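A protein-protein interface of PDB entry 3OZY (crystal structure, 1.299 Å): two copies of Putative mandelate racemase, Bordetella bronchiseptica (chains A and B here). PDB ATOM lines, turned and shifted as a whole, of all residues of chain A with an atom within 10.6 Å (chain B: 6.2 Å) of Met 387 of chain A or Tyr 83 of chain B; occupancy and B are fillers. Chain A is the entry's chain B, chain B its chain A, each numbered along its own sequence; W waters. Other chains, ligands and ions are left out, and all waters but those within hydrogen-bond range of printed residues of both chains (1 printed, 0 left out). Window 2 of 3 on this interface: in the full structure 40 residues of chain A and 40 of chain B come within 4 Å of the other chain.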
ATOM      1  N   GLY A  26     -20.723   1.980   7.151  1.00  0.00           N
ATOM      2  CA  GLY A  26     -21.055   0.600   6.832  1.00  0.00           C
ATOM      3  C   GLY A  26     -21.282   0.351   5.347  1.00  0.00           C
ATOM      4  O   GLY A  26     -21.210  -0.791   4.890  1.00  0.00           O
ATOM      5  N   ALA A  27     -21.574   1.403   4.583  1.00  0.00           N
ATOM      6  CA  ALA A  27     -21.781   1.255   3.145  1.00  0.00           C
ATOM      7  C   ALA A  27     -20.473   1.102   2.370  1.00  0.00           C
ATOM      8  O   ALA A  27     -20.493   0.753   1.189  1.00  0.00           O
ATOM      9  CB  ALA A  27     -22.579   2.427   2.603  1.00  0.00           C
ATOM     10  N   TRP A 148     -17.025   7.638  10.410  1.00  0.00           N
ATOM     11  CA  TRP A 148     -16.184   6.804  11.260  1.00  0.00           C
ATOM     12  C   TRP A 148     -14.770   7.377  11.392  1.00  0.00           C
ATOM     13  O   TRP A 148     -14.429   8.369  10.745  1.00  0.00           O
ATOM     14  CB  TRP A 148     -16.075   5.409  10.650  1.00  0.00           C
ATOM     15  CG  TRP A 148     -17.318   4.569  10.723  1.00  0.00           C
ATOM     16  CD1 TRP A 148     -18.507   4.883  11.332  1.00  0.00           C
ATOM     17  CD2 TRP A 148     -17.478   3.256  10.179  1.00  0.00           C
ATOM     18  NE1 TRP A 148     -19.397   3.836  11.188  1.00  0.00           N
ATOM     19  CE2 TRP A 148     -18.786   2.826  10.487  1.00  0.00           C
ATOM     20  CE3 TRP A 148     -16.635   2.399   9.460  1.00  0.00           C
ATOM     21  CZ2 TRP A 148     -19.268   1.570  10.107  1.00  0.00           C
ATOM     22  CZ3 TRP A 148     -17.116   1.157   9.074  1.00  0.00           C
ATOM     23  CH2 TRP A 148     -18.423   0.755   9.397  1.00  0.00           C
ATOM     24  N   GLY A 175     -21.423   1.879  14.168  1.00  0.00           N
ATOM     25  CA  GLY A 175     -21.635   0.475  13.873  1.00  0.00           C
ATOM     26  C   GLY A 175     -20.404  -0.401  13.825  1.00  0.00           C
ATOM     27  O   GLY A 175     -20.515  -1.617  13.963  1.00  0.00           O
ATOM     28  N   ALA A 202     -26.417   3.519  11.477  1.00  0.00           N
ATOM     29  CA  ALA A 202     -25.553   2.345  11.574  1.00  0.00           C
ATOM     30  C   ALA A 202     -25.328   1.631  10.241  1.00  0.00           C
ATOM     31  O   ALA A 202     -24.585   0.664  10.199  1.00  0.00           O
ATOM     32  CB  ALA A 202     -26.118   1.353  12.607  1.00  0.00           C
ATOM     33  N   ASN A 203     -25.981   2.073   9.165  1.00  0.00           N
ATOM     34  CA  ASN A 203     -25.808   1.433   7.849  1.00  0.00           C
ATOM     35  C   ASN A 203     -25.934  -0.089   7.886  1.00  0.00           C
ATOM     36  O   ASN A 203     -25.149  -0.794   7.243  1.00  0.00           O
ATOM     37  CB  ASN A 203     -24.457   1.822   7.208  1.00  0.00           C
ATOM     38  CG  ASN A 203     -24.449   3.240   6.687  1.00  0.00           C
ATOM     39  OD1 ASN A 203     -24.009   4.159   7.376  1.00  0.00           O
ATOM     40  ND2 ASN A 203     -24.932   3.427   5.457  1.00  0.00           N
ATOM     41  N   GLN A 204     -26.927  -0.586   8.627  1.00  0.00           N
ATOM     42  CA  GLN A 204     -27.239  -2.022   8.689  1.00  0.00           C
ATOM     43  C   GLN A 204     -26.153  -2.863   9.350  1.00  0.00           C
ATOM     44  O   GLN A 204     -26.088  -4.071   9.126  1.00  0.00           O
ATOM     45  CB  GLN A 204     -27.500  -2.603   7.286  1.00  0.00           C
ATOM     46  CG  GLN A 204     -28.464  -1.807   6.403  1.00  0.00           C
ATOM     47  CD  GLN A 204     -28.767  -2.532   5.093  1.00  0.00           C
ATOM     48  OE1 GLN A 204     -29.246  -3.664   5.101  1.00  0.00           O
ATOM     49  NE2 GLN A 204     -28.471  -1.890   3.958  1.00  0.00           N
ATOM     50  N   SER A 205     -25.316  -2.233  10.166  1.00  0.00           N
ATOM     51  CA  SER A 205     -24.107  -2.884  10.671  1.00  0.00           C
ATOM     52  C   SER A 205     -24.316  -3.786  11.876  1.00  0.00           C
ATOM     53  O   SER A 205     -23.478  -4.638  12.158  1.00  0.00           O
ATOM     54  CB  SER A 205     -23.038  -1.841  11.012  1.00  0.00           C
ATOM     55  OG  SER A 205     -22.583  -1.188   9.841  1.00  0.00           O
ATOM     56  N   LEU A 206     -25.417  -3.597  12.588  1.00  0.00           N
ATOM     57  CA  LEU A 206     -25.602  -4.265  13.875  1.00  0.00           C
ATOM     58  C   LEU A 206     -26.579  -5.419  13.814  1.00  0.00           C
ATOM     59  O   LEU A 206     -27.507  -5.416  13.003  1.00  0.00           O
ATOM     60  CB  LEU A 206     -26.111  -3.270  14.919  1.00  0.00           C
ATOM     61  CG  LEU A 206     -25.240  -2.039  15.150  1.00  0.00           C
ATOM     62  CD1 LEU A 206     -25.981  -1.047  16.040  1.00  0.00           C
ATOM     63  CD2 LEU A 206     -23.895  -2.425  15.762  1.00  0.00           C
ATOM     64  N   GLY A 207     -26.370  -6.399  14.687  1.00  0.00           N
ATOM     65  CA  GLY A 207     -27.386  -7.394  14.971  1.00  0.00           C
ATOM     66  C   GLY A 207     -28.348  -6.896  16.037  1.00  0.00           C
ATOM     67  O   GLY A 207     -28.145  -5.833  16.625  1.00  0.00           O
ATOM     68  N   SER A 231     -29.946  -4.912   9.365  1.00  0.00           N
ATOM     69  CA  SER A 231     -30.268  -5.297   7.994  1.00  0.00           C
ATOM     70  C   SER A 231     -31.691  -4.877   7.640  1.00  0.00           C
ATOM     71  O   SER A 231     -32.627  -5.115   8.411  1.00  0.00           O
ATOM     72  CB  SER A 231     -30.178  -6.812   7.867  1.00  0.00           C
ATOM     73  OG  SER A 231     -30.765  -7.250   6.650  1.00  0.00           O
ATOM     74  N   ALA A 383     -15.768  -1.960  -0.725  1.00  0.00           N
ATOM     75  CA  ALA A 383     -16.678  -3.012  -0.289  1.00  0.00           C
ATOM     76  C   ALA A 383     -17.396  -2.599   0.979  1.00  0.00           C
ATOM     77  O   ALA A 383     -16.779  -2.083   1.918  1.00  0.00           O
ATOM     78  CB  ALA A 383     -15.914  -4.310  -0.065  1.00  0.00           C
ATOM     79  N   GLY A 384     -18.707  -2.815   1.006  1.00  0.00           N
ATOM     80  CA  GLY A 384     -19.497  -2.526   2.183  1.00  0.00           C
ATOM     81  C   GLY A 384     -19.356  -3.579   3.263  1.00  0.00           C
ATOM     82  O   GLY A 384     -18.660  -4.587   3.098  1.00  0.00           O
ATOM     83  N   HIS A 385     -20.040  -3.340   4.374  1.00  0.00           N
ATOM     84  CA  HIS A 385     -19.916  -4.192   5.544  1.00  0.00           C
ATOM     85  C   HIS A 385     -21.205  -4.965   5.784  1.00  0.00           C
ATOM     86  O   HIS A 385     -22.206  -4.738   5.106  1.00  0.00           O
ATOM     87  CB  HIS A 385     -19.563  -3.338   6.765  1.00  0.00           C
ATOM     88  CG  HIS A 385     -18.306  -2.542   6.597  1.00  0.00           C
ATOM     89  ND1 HIS A 385     -17.089  -2.959   7.091  1.00  0.00           N
ATOM     90  CD2 HIS A 385     -18.075  -1.357   5.979  1.00  0.00           C
ATOM     91  CE1 HIS A 385     -16.163  -2.065   6.792  1.00  0.00           C
ATOM     92  NE2 HIS A 385     -16.735  -1.084   6.114  1.00  0.00           N
ATOM     93  N   GLY A 386     -21.175  -5.888   6.738  1.00  0.00           N
ATOM     94  CA  GLY A 386     -22.376  -6.598   7.139  1.00  0.00           C
ATOM     95  C   GLY A 386     -22.155  -8.089   7.241  1.00  0.00           C
ATOM     96  O   GLY A 386     -22.980  -8.825   7.789  1.00  0.00           O
ATOM     97  N   MET A 387     -21.023  -8.534   6.711  1.00  0.00           N
ATOM     98  CA  MET A 387     -20.688  -9.949   6.694  1.00  0.00           C
ATOM     99  C   MET A 387     -20.297 -10.439   8.084  1.00  0.00           C
ATOM    100  O   MET A 387     -20.671 -11.540   8.491  1.00  0.00           O
ATOM    101  CB  MET A 387     -19.550 -10.197   5.707  1.00  0.00           C
ATOM    102  CG  MET A 387     -19.331 -11.647   5.363  1.00  0.00           C
ATOM    103  SD  MET A 387     -17.941 -11.837   4.241  1.00  0.00           S
ATOM    104  CE  MET A 387     -18.012 -13.594   3.949  1.00  0.00           C
ATOM    105  N   GLU B  76      -9.484 -15.355  -5.296  1.00  0.00           N
ATOM    106  CA  GLU B  76     -10.032 -16.110  -4.174  1.00  0.00           C
ATOM    107  C   GLU B  76     -10.044 -17.613  -4.425  1.00  0.00           C
ATOM    108  O   GLU B  76     -10.157 -18.064  -5.559  1.00  0.00           O
ATOM    109  CB  GLU B  76     -11.461 -15.646  -3.869  1.00  0.00           C
ATOM    110  CG  GLU B  76     -11.556 -14.236  -3.301  1.00  0.00           C
ATOM    111  CD  GLU B  76     -11.299 -14.184  -1.807  1.00  0.00           C
ATOM    112  OE1 GLU B  76     -11.169 -15.264  -1.188  1.00  0.00           O
ATOM    113  OE2 GLU B  76     -11.235 -13.065  -1.249  1.00  0.00           O
ATOM    114  N   ASP B  77      -9.948 -18.381  -3.346  1.00  0.00           N
ATOM    115  CA  ASP B  77     -10.141 -19.823  -3.396  1.00  0.00           C
ATOM    116  C   ASP B  77     -11.628 -20.126  -3.667  1.00  0.00           C
ATOM    117  O   ASP B  77     -12.487 -19.795  -2.853  1.00  0.00           O
ATOM    118  CB  ASP B  77      -9.711 -20.414  -2.052  1.00  0.00           C
ATOM    119  CG  ASP B  77      -9.808 -21.919  -2.005  1.00  0.00           C
ATOM    120  OD1 ASP B  77     -10.374 -22.528  -2.932  1.00  0.00           O
ATOM    121  OD2 ASP B  77      -9.307 -22.502  -1.017  1.00  0.00           O
ATOM    122  N   ASN B  80     -14.364 -21.972  -1.052  1.00  0.00           N
ATOM    123  CA  ASN B  80     -15.102 -21.303   0.023  1.00  0.00           C
ATOM    124  C   ASN B  80     -16.359 -20.632  -0.511  1.00  0.00           C
ATOM    125  O   ASN B  80     -16.489 -19.406  -0.466  1.00  0.00           O
ATOM    126  CB  ASN B  80     -14.219 -20.251   0.694  1.00  0.00           C
ATOM    127  CG  ASN B  80     -12.949 -20.830   1.264  1.00  0.00           C
ATOM    128  OD1 ASN B  80     -12.948 -21.930   1.817  1.00  0.00           O
ATOM    129  ND2 ASN B  80     -11.852 -20.086   1.131  1.00  0.00           N
ATOM    130  N   ILE B  81     -17.286 -21.439  -1.016  1.00  0.00           N
ATOM    131  CA  ILE B  81     -18.495 -20.898  -1.627  1.00  0.00           C
ATOM    132  C   ILE B  81     -19.296 -20.101  -0.610  1.00  0.00           C
ATOM    133  O   ILE B  81     -19.808 -19.023  -0.914  1.00  0.00           O
ATOM    134  CB  ILE B  81     -19.375 -22.001  -2.236  1.00  0.00           C
ATOM    135  CG1 ILE B  81     -18.566 -22.842  -3.227  1.00  0.00           C
ATOM    136  CG2 ILE B  81     -20.589 -21.376  -2.936  1.00  0.00           C
ATOM    137  CD1 ILE B  81     -19.390 -23.912  -3.940  1.00  0.00           C
ATOM    138  N   ASN B  82     -19.385 -20.614   0.611  1.00  0.00           N
ATOM    139  CA  ASN B  82     -20.130 -19.907   1.649  1.00  0.00           C
ATOM    140  C   ASN B  82     -19.557 -18.524   1.955  1.00  0.00           C
ATOM    141  O   ASN B  82     -20.294 -17.525   2.000  1.00  0.00           O
ATOM    142  CB  ASN B  82     -20.217 -20.766   2.907  1.00  0.00           C
ATOM    143  CG  ASN B  82     -21.102 -21.973   2.705  1.00  0.00           C
ATOM    144  OD1 ASN B  82     -22.258 -21.839   2.304  1.00  0.00           O
ATOM    145  ND2 ASN B  82     -20.574 -23.157   2.972  1.00  0.00           N
ATOM    146  N   TYR B  83     -18.241 -18.457   2.148  1.00  0.00           N
ATOM    147  CA  TYR B  83     -17.584 -17.174   2.344  1.00  0.00           C
ATOM    148  C   TYR B  83     -17.859 -16.235   1.170  1.00  0.00           C
ATOM    149  O   TYR B  83     -18.211 -15.072   1.361  1.00  0.00           O
ATOM    150  CB  TYR B  83     -16.075 -17.376   2.520  1.00  0.00           C
ATOM    151  CG  TYR B  83     -15.288 -16.087   2.470  1.00  0.00           C
ATOM    152  CD1 TYR B  83     -15.372 -15.165   3.503  1.00  0.00           C
ATOM    153  CD2 TYR B  83     -14.460 -15.791   1.393  1.00  0.00           C
ATOM    154  CE1 TYR B  83     -14.667 -13.978   3.465  1.00  0.00           C
ATOM    155  CE2 TYR B  83     -13.739 -14.601   1.351  1.00  0.00           C
ATOM    156  CZ  TYR B  83     -13.852 -13.703   2.388  1.00  0.00           C
ATOM    157  OH  TYR B  83     -13.149 -12.517   2.360  1.00  0.00           O
ATOM    158  N   LEU B  84     -17.703 -16.743  -0.049  1.00  0.00           N
ATOM    159  CA  LEU B  84     -17.817 -15.889  -1.230  1.00  0.00           C
ATOM    160  C   LEU B  84     -19.229 -15.347  -1.448  1.00  0.00           C
ATOM    161  O   LEU B  84     -19.394 -14.214  -1.923  1.00  0.00           O
ATOM    162  CB  LEU B  84     -17.310 -16.621  -2.475  1.00  0.00           C
ATOM    163  CG  LEU B  84     -15.803 -16.889  -2.448  1.00  0.00           C
ATOM    164  CD1 LEU B  84     -15.409 -17.802  -3.599  1.00  0.00           C
ATOM    165  CD2 LEU B  84     -15.005 -15.589  -2.494  1.00  0.00           C
ATOM    166  N   TRP B  85     -20.246 -16.126  -1.075  1.00  0.00           N
ATOM    167  CA  TRP B  85     -21.626 -15.652  -1.189  1.00  0.00           C
ATOM    168  C   TRP B  85     -21.788 -14.380  -0.371  1.00  0.00           C
ATOM    169  O   TRP B  85     -22.308 -13.366  -0.843  1.00  0.00           O
ATOM    170  CB  TRP B  85     -22.618 -16.715  -0.697  1.00  0.00           C
ATOM    171  CG  TRP B  85     -24.025 -16.422  -1.143  1.00  0.00           C
ATOM    172  CD1 TRP B  85     -24.651 -16.925  -2.251  1.00  0.00           C
ATOM    173  CD2 TRP B  85     -24.962 -15.524  -0.524  1.00  0.00           C
ATOM    174  NE1 TRP B  85     -25.918 -16.408  -2.351  1.00  0.00           N
ATOM    175  CE2 TRP B  85     -26.137 -15.548  -1.305  1.00  0.00           C
ATOM    176  CE3 TRP B  85     -24.930 -14.720   0.623  1.00  0.00           C
ATOM    177  CZ2 TRP B  85     -27.264 -14.794  -0.986  1.00  0.00           C
ATOM    178  CZ3 TRP B  85     -26.061 -13.965   0.941  1.00  0.00           C
ATOM    179  CH2 TRP B  85     -27.209 -14.010   0.136  1.00  0.00           C
ATOM    180  N   HIS B  86     -21.331 -14.443   0.872  1.00  0.00           N
ATOM    181  CA  HIS B  86     -21.490 -13.325   1.788  1.00  0.00           C
ATOM    182  C   HIS B  86     -20.572 -12.157   1.469  1.00  0.00           C
ATOM    183  O   HIS B  86     -20.980 -10.996   1.581  1.00  0.00           O
ATOM    184  CB  HIS B  86     -21.389 -13.831   3.226  1.00  0.00           C
ATOM    185  CG  HIS B  86     -22.518 -14.743   3.575  1.00  0.00           C
ATOM    186  ND1 HIS B  86     -23.691 -14.285   4.129  1.00  0.00           N
ATOM    187  CD2 HIS B  86     -22.706 -16.064   3.345  1.00  0.00           C
ATOM    188  CE1 HIS B  86     -24.531 -15.291   4.281  1.00  0.00           C
ATOM    189  NE2 HIS B  86     -23.962 -16.382   3.805  1.00  0.00           N
ATOM    190  N   LYS B  87     -19.364 -12.452   1.005  1.00  0.00           N
ATOM    191  CA  LYS B  87     -18.464 -11.399   0.569  1.00  0.00           C
ATOM    192  C   LYS B  87     -19.139 -10.574  -0.531  1.00  0.00           C
ATOM    193  O   LYS B  87     -19.099  -9.339  -0.520  1.00  0.00           O
ATOM    194  CB  LYS B  87     -17.155 -12.000   0.050  1.00  0.00           C
ATOM    195  CG  LYS B  87     -16.149 -10.947  -0.354  1.00  0.00           C
ATOM    196  CD  LYS B  87     -14.889 -11.532  -0.963  1.00  0.00           C
ATOM    197  CE  LYS B  87     -13.887 -10.405  -1.202  1.00  0.00           C
ATOM    198  NZ  LYS B  87     -12.735 -10.818  -2.049  1.00  0.00           N
ATOM    199  N   VAL B  88     -19.772 -11.257  -1.478  1.00  0.00           N
ATOM    200  CA  VAL B  88     -20.410 -10.582  -2.606  1.00  0.00           C
ATOM    201  C   VAL B  88     -21.687  -9.841  -2.197  1.00  0.00           C
ATOM    202  O   VAL B  88     -21.899  -8.686  -2.577  1.00  0.00           O
ATOM    203  CB  VAL B  88     -20.696 -11.591  -3.732  1.00  0.00           C
ATOM    204  CG1 VAL B  88     -21.636 -11.003  -4.785  1.00  0.00           C
ATOM    205  CG2 VAL B  88     -19.388 -12.050  -4.371  1.00  0.00           C
ATOM    206  N   HIS B  90     -22.794  -8.724   0.872  1.00  0.00           N
ATOM    207  CA  HIS B  90     -22.579  -7.594   1.774  1.00  0.00           C
ATOM    208  C   HIS B  90     -21.609  -6.569   1.200  1.00  0.00           C
ATOM    209  O   HIS B  90     -21.724  -5.373   1.481  1.00  0.00           O
ATOM    210  CB  HIS B  90     -22.083  -8.079   3.139  1.00  0.00           C
ATOM    211  CG  HIS B  90     -23.072  -8.940   3.850  1.00  0.00           C
ATOM    212  ND1 HIS B  90     -24.235  -8.433   4.390  1.00  0.00           N
ATOM    213  CD2 HIS B  90     -23.093 -10.271   4.088  1.00  0.00           C
ATOM    214  CE1 HIS B  90     -24.926  -9.415   4.937  1.00  0.00           C
ATOM    215  NE2 HIS B  90     -24.256 -10.539   4.767  1.00  0.00           N
HETATM  216  O   HOH W   1     -25.224  -5.808   4.619  1.00  0.00           O
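Water W1 lies within hydrogen-bond range of ND1 of His 90 of chain B and O of His 385 of chain A.
The side-chain carboxylate (OE2) of Glu 76 of chain B is in salt-bridge range of the side-chain amino group (NZ) of Lys 87 of chain B (2.8 Å). The backbone NH of His 385 of chain A lies within hydrogen-bond range of the backbone carbonyl oxygen of Gly 26 of chain A, at 2.9 Å.
No position is printed for both chains. Of the 7 pairs that touch across the chains among the printed residues, none has its exchanged pair printed and touching as well.
The side-chain sulfur (SD) of Met 387 of chain A lies close to the backbone NH (N) of Lys 87 of chain B (3.6 Å).
O of His 90 of chain B touches C of Gly 384 of chain A (3.5 Å). His 385 of chain A touches His 90 of chain B. Gly 386 of chain A touches His 90 of chain B. O of Tyr 83 of chain B touches CE of Met 387 of chain A (3.0 Å). CB of His 86 of chain B touches CE of Met 387 of chain A, 3.5 Å away. Met 387 of chain A touches His 90 of chain B (N to CG, 3.5 Å).
Printed residues of chain B that touch a printed residue of chain A: Tyr 83, His 86, Lys 87 and His 90. Hydrophobic or aromatic side chains of chain B that line the printed part of chain A: Tyr 83, His 86 and His 90. Of the 16 printed residues of chain A, 4 touch a printed residue of chain B. Among the printed residues, 7 pairs touch across the chains.
Met 387 of chain A touches just these residues of chain B: Tyr 83, His 86, Lys 87 and His 90. Of chain A, only Met 387 comes within 4 Å of Tyr 83 of chain B. No residue of chain A comes within 4 Å of Asn 80 of chain B. No residue of chain A comes within 4 Å of Asn 82 of chain B. No residue of chain A comes within 4 Å of Leu 84 of chain B. Of the printed residues of chain A, Lys 87 of chain B touches Met 387 (3.4 Å). Of the printed residues of chain B, His 385 of chain A touches His 90 (3.7 Å). Of the printed residues of chain B, Gly 384 of chain A touches His 90 (3.5 Å). Printed residues of chain B within 4 Å of Gly 386 of chain A: His 90 (3.5 Å). Glu 76 of chain B touches none of the printed residues of chain A. The nearest residue of chain A that does not touch Tyr 83 of chain B is Ala 383 of chain A (9.0 Å). The nearest printed residue of chain B that does not touch Gly 386 of chain A is His 86 of chain B (6.5 Å).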
